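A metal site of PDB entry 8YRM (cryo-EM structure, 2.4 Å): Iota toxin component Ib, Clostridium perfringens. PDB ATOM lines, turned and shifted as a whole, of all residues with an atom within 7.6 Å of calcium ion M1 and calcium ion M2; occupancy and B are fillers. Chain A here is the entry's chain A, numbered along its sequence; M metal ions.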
ATOM      1  N   LEU A   3      24.584 -11.192  -2.753  1.00  0.00           N
ATOM      2  CA  LEU A   3      23.756 -12.167  -3.432  1.00  0.00           C
ATOM      3  C   LEU A   3      24.261 -13.555  -3.046  1.00  0.00           C
ATOM      4  O   LEU A   3      25.424 -13.865  -3.290  1.00  0.00           O
ATOM      5  CB  LEU A   3      23.805 -11.942  -4.944  1.00  0.00           C
ATOM      6  CG  LEU A   3      23.093 -12.995  -5.795  1.00  0.00           C
ATOM      7  CD1 LEU A   3      21.616 -13.071  -5.426  1.00  0.00           C
ATOM      8  CD2 LEU A   3      23.267 -12.678  -7.270  1.00  0.00           C
ATOM      9  N   ASP A   4      23.386 -14.347  -2.447  1.00  0.00           N
ATOM     10  CA  ASP A   4      23.751 -15.648  -1.913  1.00  0.00           C
ATOM     11  C   ASP A   4      22.841 -16.697  -2.546  1.00  0.00           C
ATOM     12  O   ASP A   4      21.828 -17.089  -1.960  1.00  0.00           O
ATOM     13  CB  ASP A   4      23.670 -15.627  -0.401  1.00  0.00           C
ATOM     14  CG  ASP A   4      24.341 -16.791   0.310  1.00  0.00           C
ATOM     15  OD1 ASP A   4      25.064 -17.535  -0.370  1.00  0.00           O
ATOM     16  OD2 ASP A   4      24.124 -16.933   1.532  1.00  0.00           O
ATOM     17  N   THR A   5      23.228 -17.166  -3.732  1.00  0.00           N
ATOM     18  CA  THR A   5      22.386 -18.065  -4.495  1.00  0.00           C
ATOM     19  C   THR A   5      22.143 -19.375  -3.745  1.00  0.00           C
ATOM     20  O   THR A   5      21.036 -19.903  -3.794  1.00  0.00           O
ATOM     21  CB  THR A   5      23.030 -18.347  -5.850  1.00  0.00           C
ATOM     22  OG1 THR A   5      23.247 -17.069  -6.425  1.00  0.00           O
ATOM     23  CG2 THR A   5      22.140 -19.219  -6.723  1.00  0.00           C
ATOM     24  N   ASP A   6      23.165 -19.898  -3.064  1.00  0.00           N
ATOM     25  CA  ASP A   6      23.064 -21.183  -2.387  1.00  0.00           C
ATOM     26  C   ASP A   6      22.624 -21.007  -0.938  1.00  0.00           C
ATOM     27  O   ASP A   6      22.403 -22.010  -0.254  1.00  0.00           O
ATOM     28  CB  ASP A   6      24.372 -21.952  -2.478  1.00  0.00           C
ATOM     29  CG  ASP A   6      25.615 -21.207  -2.025  1.00  0.00           C
ATOM     30  OD1 ASP A   6      25.495 -20.008  -1.691  1.00  0.00           O
ATOM     31  OD2 ASP A   6      26.683 -21.809  -2.039  1.00  0.00           O
ATOM     32  N   ASN A   7      22.515 -19.759  -0.479  1.00  0.00           N
ATOM     33  CA  ASN A   7      22.028 -19.438   0.854  1.00  0.00           C
ATOM     34  C   ASN A   7      22.920 -20.076   1.917  1.00  0.00           C
ATOM     35  O   ASN A   7      22.425 -20.735   2.831  1.00  0.00           O
ATOM     36  CB  ASN A   7      20.582 -19.865   1.056  1.00  0.00           C
ATOM     37  CG  ASN A   7      19.673 -19.298  -0.009  1.00  0.00           C
ATOM     38  OD1 ASN A   7      19.601 -18.076  -0.172  1.00  0.00           O
ATOM     39  ND2 ASN A   7      18.990 -20.169  -0.742  1.00  0.00           N
ATOM     40  N   ASP A   8      24.237 -19.867   1.819  1.00  0.00           N
ATOM     41  CA  ASP A   8      25.167 -20.425   2.782  1.00  0.00           C
ATOM     42  C   ASP A   8      25.918 -19.324   3.526  1.00  0.00           C
ATOM     43  O   ASP A   8      26.967 -19.581   4.087  1.00  0.00           O
ATOM     44  CB  ASP A   8      26.143 -21.380   2.115  1.00  0.00           C
ATOM     45  CG  ASP A   8      27.138 -20.752   1.155  1.00  0.00           C
ATOM     46  OD1 ASP A   8      26.883 -19.617   0.676  1.00  0.00           O
ATOM     47  OD2 ASP A   8      28.154 -21.398   0.870  1.00  0.00           O
ATOM     48  N   ASN A   9      25.384 -18.093   3.517  1.00  0.00           N
ATOM     49  CA  ASN A   9      25.935 -16.966   4.252  1.00  0.00           C
ATOM     50  C   ASN A   9      27.248 -16.462   3.661  1.00  0.00           C
ATOM     51  O   ASN A   9      27.932 -15.679   4.317  1.00  0.00           O
ATOM     52  CB  ASN A   9      26.163 -17.252   5.735  1.00  0.00           C
ATOM     53  CG  ASN A   9      24.884 -17.650   6.433  1.00  0.00           C
ATOM     54  OD1 ASN A   9      23.812 -17.131   6.115  1.00  0.00           O
ATOM     55  ND2 ASN A   9      24.982 -18.582   7.376  1.00  0.00           N
ATOM     56  N   ILE A  10      27.590 -16.857   2.431  1.00  0.00           N
ATOM     57  CA  ILE A  10      28.740 -16.274   1.754  1.00  0.00           C
ATOM     58  C   ILE A  10      28.277 -15.779   0.392  1.00  0.00           C
ATOM     59  O   ILE A  10      27.779 -16.568  -0.410  1.00  0.00           O
ATOM     60  CB  ILE A  10      29.889 -17.282   1.596  1.00  0.00           C
ATOM     61  CG1 ILE A  10      30.110 -18.079   2.873  1.00  0.00           C
ATOM     62  CG2 ILE A  10      31.176 -16.591   1.138  1.00  0.00           C
ATOM     63  CD1 ILE A  10      30.977 -19.302   2.654  1.00  0.00           C
ATOM     64  N   PRO A  11      28.398 -14.461   0.098  1.00  0.00           N
ATOM     65  CA  PRO A  11      27.974 -13.931  -1.205  1.00  0.00           C
ATOM     66  C   PRO A  11      28.673 -14.630  -2.361  1.00  0.00           C
ATOM     67  O   PRO A  11      29.805 -15.095  -2.218  1.00  0.00           O
ATOM     68  CB  PRO A  11      28.367 -12.450  -1.117  1.00  0.00           C
ATOM     69  CG  PRO A  11      28.374 -12.160   0.352  1.00  0.00           C
ATOM     70  CD  PRO A  11      28.899 -13.417   1.003  1.00  0.00           C
ATOM     71  N   ASP A  12      28.009 -14.639  -3.519  1.00  0.00           N
ATOM     72  CA  ASP A  12      28.523 -15.290  -4.707  1.00  0.00           C
ATOM     73  C   ASP A  12      29.843 -14.667  -5.132  1.00  0.00           C
ATOM     74  O   ASP A  12      30.773 -15.392  -5.504  1.00  0.00           O
ATOM     75  CB  ASP A  12      27.510 -15.211  -5.847  1.00  0.00           C
ATOM     76  CG  ASP A  12      26.202 -15.919  -5.560  1.00  0.00           C
ATOM     77  OD1 ASP A  12      26.092 -16.542  -4.469  1.00  0.00           O
ATOM     78  OD2 ASP A  12      25.294 -15.829  -6.419  1.00  0.00           O
ATOM     79  N   ALA A  13      29.930 -13.340  -5.076  1.00  0.00           N
ATOM     80  CA  ALA A  13      31.143 -12.655  -5.488  1.00  0.00           C
ATOM     81  C   ALA A  13      32.300 -13.096  -4.606  1.00  0.00           C
ATOM     82  O   ALA A  13      33.423 -13.270  -5.087  1.00  0.00           O
ATOM     83  CB  ALA A  13      30.931 -11.166  -5.450  1.00  0.00           C
ATOM     84  N   GLU A  15      32.594 -15.957  -2.956  1.00  0.00           N
ATOM     85  CA  GLU A  15      32.974 -17.333  -3.221  1.00  0.00           C
ATOM     86  C   GLU A  15      33.773 -17.455  -4.518  1.00  0.00           C
ATOM     87  O   GLU A  15      34.747 -18.211  -4.556  1.00  0.00           O
ATOM     88  CB  GLU A  15      31.763 -18.261  -3.268  1.00  0.00           C
ATOM     89  CG  GLU A  15      30.957 -18.271  -1.972  1.00  0.00           C
ATOM     90  CD  GLU A  15      30.161 -19.532  -1.741  1.00  0.00           C
ATOM     91  OE1 GLU A  15      30.787 -20.607  -1.637  1.00  0.00           O
ATOM     92  OE2 GLU A  15      28.930 -19.472  -1.627  1.00  0.00           O
ATOM     93  N   TYR A  19      37.684 -15.103  -0.136  1.00  0.00           N
ATOM     94  CA  TYR A  19      37.105 -14.507   1.055  1.00  0.00           C
ATOM     95  C   TYR A  19      37.762 -15.095   2.305  1.00  0.00           C
ATOM     96  O   TYR A  19      38.445 -16.106   2.241  1.00  0.00           O
ATOM     97  CB  TYR A  19      35.603 -14.728   1.079  1.00  0.00           C
ATOM     98  CG  TYR A  19      35.203 -16.178   1.238  1.00  0.00           C
ATOM     99  CD1 TYR A  19      35.072 -17.023   0.139  1.00  0.00           C
ATOM    100  CD2 TYR A  19      34.964 -16.717   2.499  1.00  0.00           C
ATOM    101  CE1 TYR A  19      34.713 -18.344   0.273  1.00  0.00           C
ATOM    102  CE2 TYR A  19      34.610 -18.055   2.656  1.00  0.00           C
ATOM    103  CZ  TYR A  19      34.490 -18.868   1.533  1.00  0.00           C
ATOM    104  OH  TYR A  19      34.117 -20.179   1.633  1.00  0.00           O
ATOM    105  N   VAL A  42      38.091 -20.167  -1.264  1.00  0.00           N
ATOM    106  CA  VAL A  42      37.216 -20.119  -2.418  1.00  0.00           C
ATOM    107  C   VAL A  42      36.289 -21.326  -2.349  1.00  0.00           C
ATOM    108  O   VAL A  42      36.624 -22.334  -1.741  1.00  0.00           O
ATOM    109  CB  VAL A  42      38.002 -20.112  -3.746  1.00  0.00           C
ATOM    110  CG1 VAL A  42      38.686 -18.771  -3.978  1.00  0.00           C
ATOM    111  CG2 VAL A  42      39.011 -21.237  -3.816  1.00  0.00           C
ATOM    112  N   SER A  43      35.111 -21.208  -2.960  1.00  0.00           N
ATOM    113  CA  SER A  43      34.141 -22.289  -2.943  1.00  0.00           C
ATOM    114  C   SER A  43      33.130 -22.065  -4.054  1.00  0.00           C
ATOM    115  O   SER A  43      33.163 -21.040  -4.737  1.00  0.00           O
ATOM    116  CB  SER A  43      33.467 -22.436  -1.595  1.00  0.00           C
ATOM    117  OG  SER A  43      33.244 -21.177  -0.974  1.00  0.00           O
ATOM    118  N   SER A  44      32.259 -23.046  -4.269  1.00  0.00           N
ATOM    119  CA  SER A  44      31.230 -22.929  -5.284  1.00  0.00           C
ATOM    120  C   SER A  44      30.086 -22.059  -4.769  1.00  0.00           C
ATOM    121  O   SER A  44      29.549 -22.305  -3.689  1.00  0.00           O
ATOM    122  CB  SER A  44      30.716 -24.282  -5.676  1.00  0.00           C
ATOM    123  OG  SER A  44      29.491 -24.144  -6.385  1.00  0.00           O
ATOM    124  N   TYR A  45      29.682 -21.077  -5.572  1.00  0.00           N
ATOM    125  CA  TYR A  45      28.578 -20.219  -5.194  1.00  0.00           C
ATOM    126  C   TYR A  45      27.240 -20.884  -5.505  1.00  0.00           C
ATOM    127  O   TYR A  45      26.206 -20.346  -5.134  1.00  0.00           O
ATOM    128  CB  TYR A  45      28.706 -18.860  -5.870  1.00  0.00           C
ATOM    129  CG  TYR A  45      28.417 -18.853  -7.356  1.00  0.00           C
ATOM    130  CD1 TYR A  45      29.432 -19.079  -8.274  1.00  0.00           C
ATOM    131  CD2 TYR A  45      27.134 -18.630  -7.839  1.00  0.00           C
ATOM    132  CE1 TYR A  45      29.180 -19.069  -9.636  1.00  0.00           C
ATOM    133  CE2 TYR A  45      26.873 -18.624  -9.201  1.00  0.00           C
ATOM    134  CZ  TYR A  45      27.905 -18.840 -10.099  1.00  0.00           C
ATOM    135  OH  TYR A  45      27.652 -18.827 -11.441  1.00  0.00           O
ATOM    136  N   LEU A  46      27.257 -22.067  -6.144  1.00  0.00           N
ATOM    137  CA  LEU A  46      26.045 -22.824  -6.431  1.00  0.00           C
ATOM    138  C   LEU A  46      25.889 -24.030  -5.507  1.00  0.00           C
ATOM    139  O   LEU A  46      24.880 -24.719  -5.564  1.00  0.00           O
ATOM    140  CB  LEU A  46      26.021 -23.248  -7.890  1.00  0.00           C
ATOM    141  CG  LEU A  46      25.740 -22.146  -8.914  1.00  0.00           C
ATOM    142  CD1 LEU A  46      25.592 -22.769 -10.292  1.00  0.00           C
ATOM    143  CD2 LEU A  46      24.517 -21.305  -8.584  1.00  0.00           C
ATOM    144  N   GLU A  47      26.879 -24.295  -4.645  1.00  0.00           N
ATOM    145  CA  GLU A  47      26.797 -25.411  -3.719  1.00  0.00           C
ATOM    146  C   GLU A  47      27.029 -24.912  -2.295  1.00  0.00           C
ATOM    147  O   GLU A  47      27.989 -24.192  -2.034  1.00  0.00           O
ATOM    148  CB  GLU A  47      27.848 -26.455  -4.072  1.00  0.00           C
ATOM    149  CG  GLU A  47      27.359 -27.464  -5.104  1.00  0.00           C
ATOM    150  CD  GLU A  47      26.268 -28.388  -4.584  1.00  0.00           C
ATOM    151  OE1 GLU A  47      26.147 -28.535  -3.333  1.00  0.00           O
ATOM    152  OE2 GLU A  47      25.528 -28.933  -5.422  1.00  0.00           O
ATOM    153  N   SER A  48      26.145 -25.307  -1.382  1.00  0.00           N
ATOM    154  CA  SER A  48      26.325 -24.960   0.010  1.00  0.00           C
ATOM    155  C   SER A  48      27.439 -25.805   0.636  1.00  0.00           C
ATOM    156  O   SER A  48      28.148 -25.357   1.528  1.00  0.00           O
ATOM    157  CB  SER A  48      25.040 -25.102   0.770  1.00  0.00           C
ATOM    158  OG  SER A  48      24.674 -26.463   0.878  1.00  0.00           O
ATOM    159  N   ASN A  49      27.567 -27.048   0.168  1.00  0.00           N
ATOM    160  CA  ASN A  49      28.573 -27.968   0.644  1.00  0.00           C
ATOM    161  C   ASN A  49      29.476 -28.371  -0.510  1.00  0.00           C
ATOM    162  O   ASN A  49      29.301 -29.436  -1.081  1.00  0.00           O
ATOM    163  CB  ASN A  49      27.924 -29.195   1.257  1.00  0.00           C
ATOM    164  CG  ASN A  49      27.051 -28.850   2.443  1.00  0.00           C
ATOM    165  OD1 ASN A  49      26.227 -27.937   2.357  1.00  0.00           O
ATOM    166  ND2 ASN A  49      27.195 -29.566   3.549  1.00  0.00           N
ATOM    167  N   THR A  50      30.464 -27.533  -0.832  1.00  0.00           N
ATOM    168  CA  THR A  50      31.296 -27.729  -2.004  1.00  0.00           C
ATOM    169  C   THR A  50      32.020 -29.081  -1.960  1.00  0.00           C
ATOM    170  O   THR A  50      32.144 -29.721  -2.999  1.00  0.00           O
ATOM    171  CB  THR A  50      32.288 -26.583  -2.119  1.00  0.00           C
ATOM    172  OG1 THR A  50      31.510 -25.404  -2.252  1.00  0.00           O
ATOM    173  CG2 THR A  50      33.222 -26.769  -3.314  1.00  0.00           C
ATOM    174  N   THR A  56      28.610 -27.050   5.753  1.00  0.00           N
ATOM    175  CA  THR A  56      28.549 -26.088   4.667  1.00  0.00           C
ATOM    176  C   THR A  56      29.872 -25.346   4.539  1.00  0.00           C
ATOM    177  O   THR A  56      30.738 -25.437   5.414  1.00  0.00           O
ATOM    178  CB  THR A  56      27.387 -25.109   4.869  1.00  0.00           C
ATOM    179  OG1 THR A  56      27.755 -24.177   5.882  1.00  0.00           O
ATOM    180  CG2 THR A  56      26.094 -25.806   5.247  1.00  0.00           C
ATOM    181  N   ASP A  57      30.011 -24.593   3.460  1.00  0.00           N
ATOM    182  CA  ASP A  57      31.197 -23.781   3.208  1.00  0.00           C
ATOM    183  C   ASP A  57      31.421 -22.780   4.341  1.00  0.00           C
ATOM    184  O   ASP A  57      32.557 -22.545   4.732  1.00  0.00           O
ATOM    185  CB  ASP A  57      31.083 -23.076   1.872  1.00  0.00           C
ATOM    186  CG  ASP A  57      30.924 -24.013   0.674  1.00  0.00           C
ATOM    187  OD1 ASP A  57      31.161 -25.223   0.828  1.00  0.00           O
ATOM    188  OD2 ASP A  57      30.552 -23.530  -0.395  1.00  0.00           O
ATOM    189  N   TYR A  58      30.346 -22.166   4.850  1.00  0.00           N
ATOM    190  CA  TYR A  58      30.468 -21.171   5.905  1.00  0.00           C
ATOM    191  C   TYR A  58      30.859 -21.850   7.218  1.00  0.00           C
ATOM    192  O   TYR A  58      31.727 -21.358   7.933  1.00  0.00           O
ATOM    193  CB  TYR A  58      29.182 -20.351   6.060  1.00  0.00           C
ATOM    194  CG  TYR A  58      29.233 -19.467   7.288  1.00  0.00           C
ATOM    195  CD1 TYR A  58      29.937 -18.265   7.262  1.00  0.00           C
ATOM    196  CD2 TYR A  58      28.669 -19.861   8.491  1.00  0.00           C
ATOM    197  CE1 TYR A  58      30.054 -17.473   8.388  1.00  0.00           C
ATOM    198  CE2 TYR A  58      28.776 -19.071   9.626  1.00  0.00           C
ATOM    199  CZ  TYR A  58      29.463 -17.878   9.580  1.00  0.00           C
ATOM    200  OH  TYR A  58      29.560 -17.087  10.684  1.00  0.00           O
ATOM    201  N   PRO A  76      37.011 -25.035   2.563  1.00  0.00           N
ATOM    202  CA  PRO A  76      35.858 -25.592   1.854  1.00  0.00           C
ATOM    203  C   PRO A  76      36.193 -26.654   0.806  1.00  0.00           C
ATOM    204  O   PRO A  76      35.363 -27.504   0.525  1.00  0.00           O
ATOM    205  CB  PRO A  76      35.187 -24.377   1.248  1.00  0.00           C
ATOM    206  CG  PRO A  76      35.589 -23.264   2.185  1.00  0.00           C
ATOM    207  CD  PRO A  76      37.023 -23.576   2.543  1.00  0.00           C
HETATM  208 CA    CA M   1      26.904 -18.586  -1.186  1.00  0.00          CA
HETATM  209 CA    CA M   2      28.858 -22.228  -1.483  1.00  0.00          CA
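Merely in contact with calcium ion M1: Asp 12 (3.95 Å).
Six residues have an atom within 4 Å of calcium ion M1: Asp 4, Asp 6, Asp 8, Ile 10, Asp 12 and Glu 15.
Calcium ion M2 is bound by O of Glu 47 (2.2 Å), OD2 of Asp 6 (2.3 Å), O of Ser 44 (2.3 Å), OD2 of Asp 57 (2.4 Å), OE1 of Glu 15 (2.5 Å), OD2 of Asp 8 (2.6 Å) and OE2 of Glu 15 (2.8 Å).
The side-chain hydroxyl of Thr 50 is in hydrogen-bond range of the backbone NH of Ser 44 (3.2 Å).
The backbone NH (N) of Glu 47 lies within hydrogen-bond range of the side-chain hydroxyl (OG) of Ser 44 (3.1 Å).
The backbone carbonyl oxygen (O) of Asp 4 sits close to the side-chain amide oxygen (OD1) of Asn 7, at 3.0 Å.
The backbone NH (N) of Asp 57 sits at hydrogen-bond distance from the backbone carbonyl oxygen (O) of Ser 48 (2.8 Å).
The side-chain carboxylate (OD1) of Asp 12 sits at hydrogen-bond distance from the backbone NH (N) of Thr 5.
The side-chain carboxylate (OD1) of Asp 57 is in hydrogen-bond range of the backbone NH (N) of Thr 50 (2.9 Å).
The backbone NH (N) of Ser 43 lies within hydrogen-bond range of the backbone carbonyl oxygen (O) of Glu 15 (3.4 Å).
The backbone carbonyl oxygen of Leu 3 sits at hydrogen-bond distance from the backbone NH of Asp 12, at 2.7 Å.
Calcium ion M1 is bound by the side-chain carboxylate (OD1) of Asp 6, the side-chain carboxylate (OD1) of Asp 8, the side-chain carboxylate (OE2) of Glu 15, the side-chain carboxylate (OD1) of Asp 4 and the backbone carbonyl oxygen (O) of Ile 10.
Of the 26 residues printed, 6 come within 4 Å of calcium ion M2.
The nearest printed residue that does not touch calcium ion M2 is Ser 48 (4.01 Å).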
